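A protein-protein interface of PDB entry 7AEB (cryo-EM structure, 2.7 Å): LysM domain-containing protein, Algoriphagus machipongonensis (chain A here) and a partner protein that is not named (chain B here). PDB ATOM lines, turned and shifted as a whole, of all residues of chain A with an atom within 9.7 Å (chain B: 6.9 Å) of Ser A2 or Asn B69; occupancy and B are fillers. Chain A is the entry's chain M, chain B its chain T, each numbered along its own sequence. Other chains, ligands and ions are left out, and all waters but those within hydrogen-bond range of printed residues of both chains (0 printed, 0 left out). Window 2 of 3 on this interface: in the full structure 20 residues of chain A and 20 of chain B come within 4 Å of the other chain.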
ATOM      1  N   SER A   2      -3.213  20.073  -9.831  1.00  0.00           N
ATOM      2  CA  SER A   2      -2.606  21.396  -9.865  1.00  0.00           C
ATOM      3  C   SER A   2      -2.628  22.046  -8.489  1.00  0.00           C
ATOM      4  O   SER A   2      -2.543  23.265  -8.373  1.00  0.00           O
ATOM      5  CB  SER A   2      -3.323  22.288 -10.878  1.00  0.00           C
ATOM      6  OG  SER A   2      -3.025  23.655 -10.655  1.00  0.00           O
ATOM      7  N   GLU A   3      -2.787  21.210  -7.467  1.00  0.00           N
ATOM      8  CA  GLU A   3      -2.641  21.640  -6.085  1.00  0.00           C
ATOM      9  C   GLU A   3      -1.199  22.012  -5.795  1.00  0.00           C
ATOM     10  O   GLU A   3      -0.920  22.979  -5.076  1.00  0.00           O
ATOM     11  CB  GLU A   3      -3.084  20.528  -5.134  1.00  0.00           C
ATOM     12  CG  GLU A   3      -3.067  20.922  -3.670  1.00  0.00           C
ATOM     13  CD  GLU A   3      -3.555  19.820  -2.751  1.00  0.00           C
ATOM     14  OE1 GLU A   3      -3.416  19.958  -1.519  1.00  0.00           O
ATOM     15  OE2 GLU A   3      -3.998  18.773  -3.271  1.00  0.00           O
ATOM     16  N   GLY A   4      -0.272  21.238  -6.360  1.00  0.00           N
ATOM     17  CA  GLY A   4       1.146  21.389  -6.134  1.00  0.00           C
ATOM     18  C   GLY A   4       1.780  22.578  -6.806  1.00  0.00           C
ATOM     19  O   GLY A   4       2.967  22.830  -6.592  1.00  0.00           O
ATOM     20  N   LYS A   5       1.023  23.313  -7.610  1.00  0.00           N
ATOM     21  CA  LYS A   5       1.533  24.494  -8.284  1.00  0.00           C
ATOM     22  C   LYS A   5       1.546  25.693  -7.347  1.00  0.00           C
ATOM     23  O   LYS A   5       0.542  25.993  -6.699  1.00  0.00           O
ATOM     24  CB  LYS A   5       0.677  24.809  -9.506  1.00  0.00           C
ATOM     25  CG  LYS A   5       1.103  26.058 -10.237  1.00  0.00           C
ATOM     26  CD  LYS A   5       0.029  26.568 -11.157  1.00  0.00           C
ATOM     27  CE  LYS A   5       0.436  27.893 -11.762  1.00  0.00           C
ATOM     28  NZ  LYS A   5      -0.551  28.368 -12.765  1.00  0.00           N
ATOM     29  N   LEU A   6       2.683  26.383  -7.290  1.00  0.00           N
ATOM     30  CA  LEU A   6       2.805  27.653  -6.583  1.00  0.00           C
ATOM     31  C   LEU A   6       2.216  28.758  -7.453  1.00  0.00           C
ATOM     32  O   LEU A   6       2.803  29.143  -8.463  1.00  0.00           O
ATOM     33  CB  LEU A   6       4.263  27.942  -6.240  1.00  0.00           C
ATOM     34  CG  LEU A   6       4.548  29.200  -5.408  1.00  0.00           C
ATOM     35  CD1 LEU A   6       3.953  29.088  -4.027  1.00  0.00           C
ATOM     36  CD2 LEU A   6       6.031  29.464  -5.312  1.00  0.00           C
ATOM     37  N   GLU A   7       1.059  29.276  -7.056  1.00  0.00           N
ATOM     38  CA  GLU A   7       0.408  30.339  -7.806  1.00  0.00           C
ATOM     39  C   GLU A   7       1.063  31.686  -7.514  1.00  0.00           C
ATOM     40  O   GLU A   7       1.515  31.950  -6.398  1.00  0.00           O
ATOM     41  CB  GLU A   7      -1.083  30.382  -7.459  1.00  0.00           C
ATOM     42  CG  GLU A   7      -1.933  31.268  -8.362  1.00  0.00           C
ATOM     43  CD  GLU A   7      -2.260  30.628  -9.704  1.00  0.00           C
ATOM     44  OE1 GLU A   7      -2.665  31.358 -10.627  1.00  0.00           O
ATOM     45  OE2 GLU A   7      -2.122  29.395  -9.840  1.00  0.00           O
ATOM     46  N   LYS A   8       1.121  32.539  -8.535  1.00  0.00           N
ATOM     47  CA  LYS A   8       1.731  33.857  -8.452  1.00  0.00           C
ATOM     48  C   LYS A   8       0.669  34.939  -8.591  1.00  0.00           C
ATOM     49  O   LYS A   8      -0.316  34.766  -9.311  1.00  0.00           O
ATOM     50  CB  LYS A   8       2.795  34.016  -9.534  1.00  0.00           C
ATOM     51  CG  LYS A   8       4.047  33.216  -9.266  1.00  0.00           C
ATOM     52  CD  LYS A   8       4.865  33.857  -8.171  1.00  0.00           C
ATOM     53  CE  LYS A   8       5.826  32.874  -7.561  1.00  0.00           C
ATOM     54  NZ  LYS A   8       6.693  32.252  -8.584  1.00  0.00           N
ATOM     55  N   THR A 117      -5.775  39.592  -8.067  1.00  0.00           N
ATOM     56  CA  THR A 117      -6.178  38.217  -7.794  1.00  0.00           C
ATOM     57  C   THR A 117      -4.984  37.365  -7.388  1.00  0.00           C
ATOM     58  O   THR A 117      -3.971  37.332  -8.091  1.00  0.00           O
ATOM     59  CB  THR A 117      -6.862  37.558  -9.005  1.00  0.00           C
ATOM     60  OG1 THR A 117      -6.087  37.775 -10.189  1.00  0.00           O
ATOM     61  CG2 THR A 117      -8.261  38.097  -9.212  1.00  0.00           C
ATOM     62  N   TRP A 118      -5.118  36.665  -6.267  1.00  0.00           N
ATOM     63  CA  TRP A 118      -4.135  35.667  -5.849  1.00  0.00           C
ATOM     64  C   TRP A 118      -4.833  34.664  -4.946  1.00  0.00           C
ATOM     65  O   TRP A 118      -5.128  34.980  -3.793  1.00  0.00           O
ATOM     66  CB  TRP A 118      -2.961  36.313  -5.123  1.00  0.00           C
ATOM     67  CG  TRP A 118      -1.953  35.341  -4.586  1.00  0.00           C
ATOM     68  CD1 TRP A 118      -1.547  34.180  -5.164  1.00  0.00           C
ATOM     69  CD2 TRP A 118      -1.215  35.460  -3.369  1.00  0.00           C
ATOM     70  NE1 TRP A 118      -0.617  33.559  -4.377  1.00  0.00           N
ATOM     71  CE2 TRP A 118      -0.392  34.326  -3.270  1.00  0.00           C
ATOM     72  CE3 TRP A 118      -1.174  36.414  -2.349  1.00  0.00           C
ATOM     73  CZ2 TRP A 118       0.461  34.116  -2.190  1.00  0.00           C
ATOM     74  CZ3 TRP A 118      -0.322  36.206  -1.283  1.00  0.00           C
ATOM     75  CH2 TRP A 118       0.484  35.066  -1.212  1.00  0.00           C
ATOM     76  N   GLY A 119      -5.072  33.461  -5.457  1.00  0.00           N
ATOM     77  CA  GLY A 119      -5.712  32.424  -4.667  1.00  0.00           C
ATOM     78  C   GLY A 119      -7.155  32.755  -4.356  1.00  0.00           C
ATOM     79  O   GLY A 119      -7.997  32.865  -5.248  1.00  0.00           O
ATOM     80  N   SER A 120      -7.434  32.948  -3.071  1.00  0.00           N
ATOM     81  CA  SER A 120      -8.747  33.322  -2.570  1.00  0.00           C
ATOM     82  C   SER A 120      -9.033  34.815  -2.673  1.00  0.00           C
ATOM     83  O   SER A 120     -10.183  35.219  -2.494  1.00  0.00           O
ATOM     84  CB  SER A 120      -8.869  32.882  -1.114  1.00  0.00           C
ATOM     85  OG  SER A 120     -10.090  33.305  -0.552  1.00  0.00           O
ATOM     86  N   PRO B  67      -7.103  24.857 -16.931  1.00  0.00           N
ATOM     87  CA  PRO B  67      -6.990  23.944 -15.779  1.00  0.00           C
ATOM     88  C   PRO B  67      -7.832  24.427 -14.614  1.00  0.00           C
ATOM     89  O   PRO B  67      -8.115  25.615 -14.486  1.00  0.00           O
ATOM     90  CB  PRO B  67      -5.497  24.025 -15.431  1.00  0.00           C
ATOM     91  CG  PRO B  67      -5.076  25.376 -15.943  1.00  0.00           C
ATOM     92  CD  PRO B  67      -5.858  25.593 -17.180  1.00  0.00           C
ATOM     93  N   ILE B  68      -8.193  23.497 -13.732  1.00  0.00           N
ATOM     94  CA  ILE B  68      -9.052  23.796 -12.594  1.00  0.00           C
ATOM     95  C   ILE B  68      -8.231  23.944 -11.317  1.00  0.00           C
ATOM     96  O   ILE B  68      -7.521  23.018 -10.916  1.00  0.00           O
ATOM     97  CB  ILE B  68     -10.139  22.729 -12.421  1.00  0.00           C
ATOM     98  CG1 ILE B  68     -10.996  22.644 -13.687  1.00  0.00           C
ATOM     99  CG2 ILE B  68     -11.008  23.024 -11.213  1.00  0.00           C
ATOM    100  CD1 ILE B  68     -11.737  21.336 -13.871  1.00  0.00           C
ATOM    101  N   ASN B  69      -8.351  25.101 -10.656  1.00  0.00           N
ATOM    102  CA  ASN B  69      -7.631  25.375  -9.419  1.00  0.00           C
ATOM    103  C   ASN B  69      -8.420  26.380  -8.580  1.00  0.00           C
ATOM    104  O   ASN B  69      -9.489  26.839  -8.981  1.00  0.00           O
ATOM    105  CB  ASN B  69      -6.213  25.867  -9.717  1.00  0.00           C
ATOM    106  CG  ASN B  69      -6.183  27.154 -10.522  1.00  0.00           C
ATOM    107  OD1 ASN B  69      -6.768  28.175 -10.156  1.00  0.00           O
ATOM    108  ND2 ASN B  69      -5.458  27.120 -11.619  1.00  0.00           N
ATOM    109  N   ARG B  70      -7.818  26.782  -7.452  1.00  0.00           N
ATOM    110  CA  ARG B  70      -8.432  27.706  -6.491  1.00  0.00           C
ATOM    111  C   ARG B  70      -8.695  29.095  -7.068  1.00  0.00           C
ATOM    112  O   ARG B  70      -9.676  29.745  -6.688  1.00  0.00           O
ATOM    113  CB  ARG B  70      -7.524  27.827  -5.266  1.00  0.00           C
ATOM    114  CG  ARG B  70      -7.910  28.872  -4.200  1.00  0.00           C
ATOM    115  CD  ARG B  70      -9.233  28.597  -3.540  1.00  0.00           C
ATOM    116  NE  ARG B  70      -9.190  27.376  -2.753  1.00  0.00           N
ATOM    117  CZ  ARG B  70     -10.246  26.801  -2.189  1.00  0.00           C
ATOM    118  NH1 ARG B  70     -11.450  27.330  -2.315  1.00  0.00           N
ATOM    119  NH2 ARG B  70     -10.093  25.687  -1.497  1.00  0.00           N
ATOM    120  N   THR B  71      -7.803  29.588  -7.931  1.00  0.00           N
ATOM    121  CA  THR B  71      -7.981  30.922  -8.489  1.00  0.00           C
ATOM    122  C   THR B  71      -9.177  30.936  -9.415  1.00  0.00           C
ATOM    123  O   THR B  71     -10.013  31.845  -9.345  1.00  0.00           O
ATOM    124  CB  THR B  71      -6.725  31.381  -9.242  1.00  0.00           C
ATOM    125  OG1 THR B  71      -5.600  31.389  -8.360  1.00  0.00           O
ATOM    126  CG2 THR B  71      -6.919  32.785  -9.770  1.00  0.00           C
ATOM    127  N   LEU B  72      -9.267  29.915 -10.279  1.00  0.00           N
ATOM    128  CA  LEU B  72     -10.425  29.750 -11.148  1.00  0.00           C
ATOM    129  C   LEU B  72     -11.714  29.704 -10.374  1.00  0.00           C
ATOM    130  O   LEU B  72     -12.656  30.421 -10.717  1.00  0.00           O
ATOM    131  CB  LEU B  72     -10.309  28.500 -12.031  1.00  0.00           C
ATOM    132  CG  LEU B  72     -11.369  28.310 -13.150  1.00  0.00           C
ATOM    133  CD1 LEU B  72     -10.797  27.682 -14.385  1.00  0.00           C
ATOM    134  CD2 LEU B  72     -12.529  27.371 -12.635  1.00  0.00           C
ATOM    135  N   LYS B  73     -11.784  28.855  -9.350  1.00  0.00           N
ATOM    136  CA  LYS B  73     -13.032  28.720  -8.609  1.00  0.00           C
ATOM    137  C   LYS B  73     -13.487  30.042  -8.017  1.00  0.00           C
ATOM    138  O   LYS B  73     -14.670  30.380  -8.105  1.00  0.00           O
ATOM    139  CB  LYS B  73     -12.882  27.685  -7.511  1.00  0.00           C
ATOM    140  CG  LYS B  73     -12.798  26.295  -8.043  1.00  0.00           C
ATOM    141  CD  LYS B  73     -12.618  25.310  -6.931  1.00  0.00           C
ATOM    142  CE  LYS B  73     -12.543  23.899  -7.465  1.00  0.00           C
ATOM    143  NZ  LYS B  73     -12.333  22.917  -6.369  1.00  0.00           N
ATOM    144  N   THR B  74     -12.544  30.840  -7.511  1.00  0.00           N
ATOM    145  CA  THR B  74     -12.880  32.149  -6.967  1.00  0.00           C
ATOM    146  C   THR B  74     -13.463  33.057  -8.040  1.00  0.00           C
ATOM    147  O   THR B  74     -14.495  33.706  -7.823  1.00  0.00           O
ATOM    148  CB  THR B  74     -11.635  32.789  -6.347  1.00  0.00           C
ATOM    149  OG1 THR B  74     -11.124  31.944  -5.313  1.00  0.00           O
ATOM    150  CG2 THR B  74     -11.971  34.134  -5.753  1.00  0.00           C
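The side-chain hydroxyl of Thr B74 is in hydrogen-bond range of the backbone carbonyl oxygen of Gly A119, at 3.3 Å.
The backbone carbonyl oxygen (O) of Arg B70 lies within hydrogen-bond range of the side-chain hydroxyl (OG1) of Thr B74, 3.0 Å away.
The indole nitrogen (NE1) of Trp A118 is in hydrogen-bond range of the backbone carbonyl oxygen (O) of Glu A7 (3.3 Å).
The side-chain amino group (NZ) of Lys A5 lies within salt-bridge range of the side-chain carboxylate (OE2) of Glu A7 (3.5 Å).
N of Thr B71 is in hydrogen-bond range of OD1 of Asn B69 (2.8 Å).
N of Leu B72 lies within hydrogen-bond range of OD1 of Asn B69, at 3.0 Å.
Among the printed residues, merely in contact across the chains: Gly A119 with Thr B71, Glu A7 with Thr B71, Gly A119 with Arg B70, Ser A120 with Thr B74 and Ser A2 with Asn B69.
Printed residues of chain B within 4 Å of Ser A2: Asn B69.
Of the printed residues of chain A, Asn B69 touches Ser A2 (3.99 Å).
Thr B71 touches two residues of chain A.
No residue of chain A comes within 4 Å of Leu B72.
Printed residues of chain A within 4 Å of Thr B74: Gly A119 (3.3 Å) and Ser A120 (3.9 Å).
Of the printed residues of chain B, Ser A120 touches Thr B74 (3.9 Å).
Printed residues of chain B within 4 Å of Gly A119: Arg B70, Thr B71 and Thr B74.
Pro B67 touches none of the printed residues of chain A.
The nearest printed residue of chain B that does not touch Ser A2 is Ile B68 (4.3 Å).
The nearest printed residue of chain A that does not touch Asn B69 is Glu A7 (4.4 Å).
The nearest printed residue of chain B that does not touch Glu A7 is Asn B69 (4.4 Å).
Of the 8 printed residues of chain B, 4 touch a printed residue of chain A.
Printed residues of chain B that touch a printed residue of chain A: Asn B69, Arg B70, Thr B71 and Thr B74.
Of the 11 printed residues of chain A, 4 touch a printed residue of chain B.
Among the printed residues, 6 pairs touch across the chains.
Among the printed residues, no Asp or Glu carboxylate lies within 4 Å of a Lys or Arg side-chain nitrogen of the other chain.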
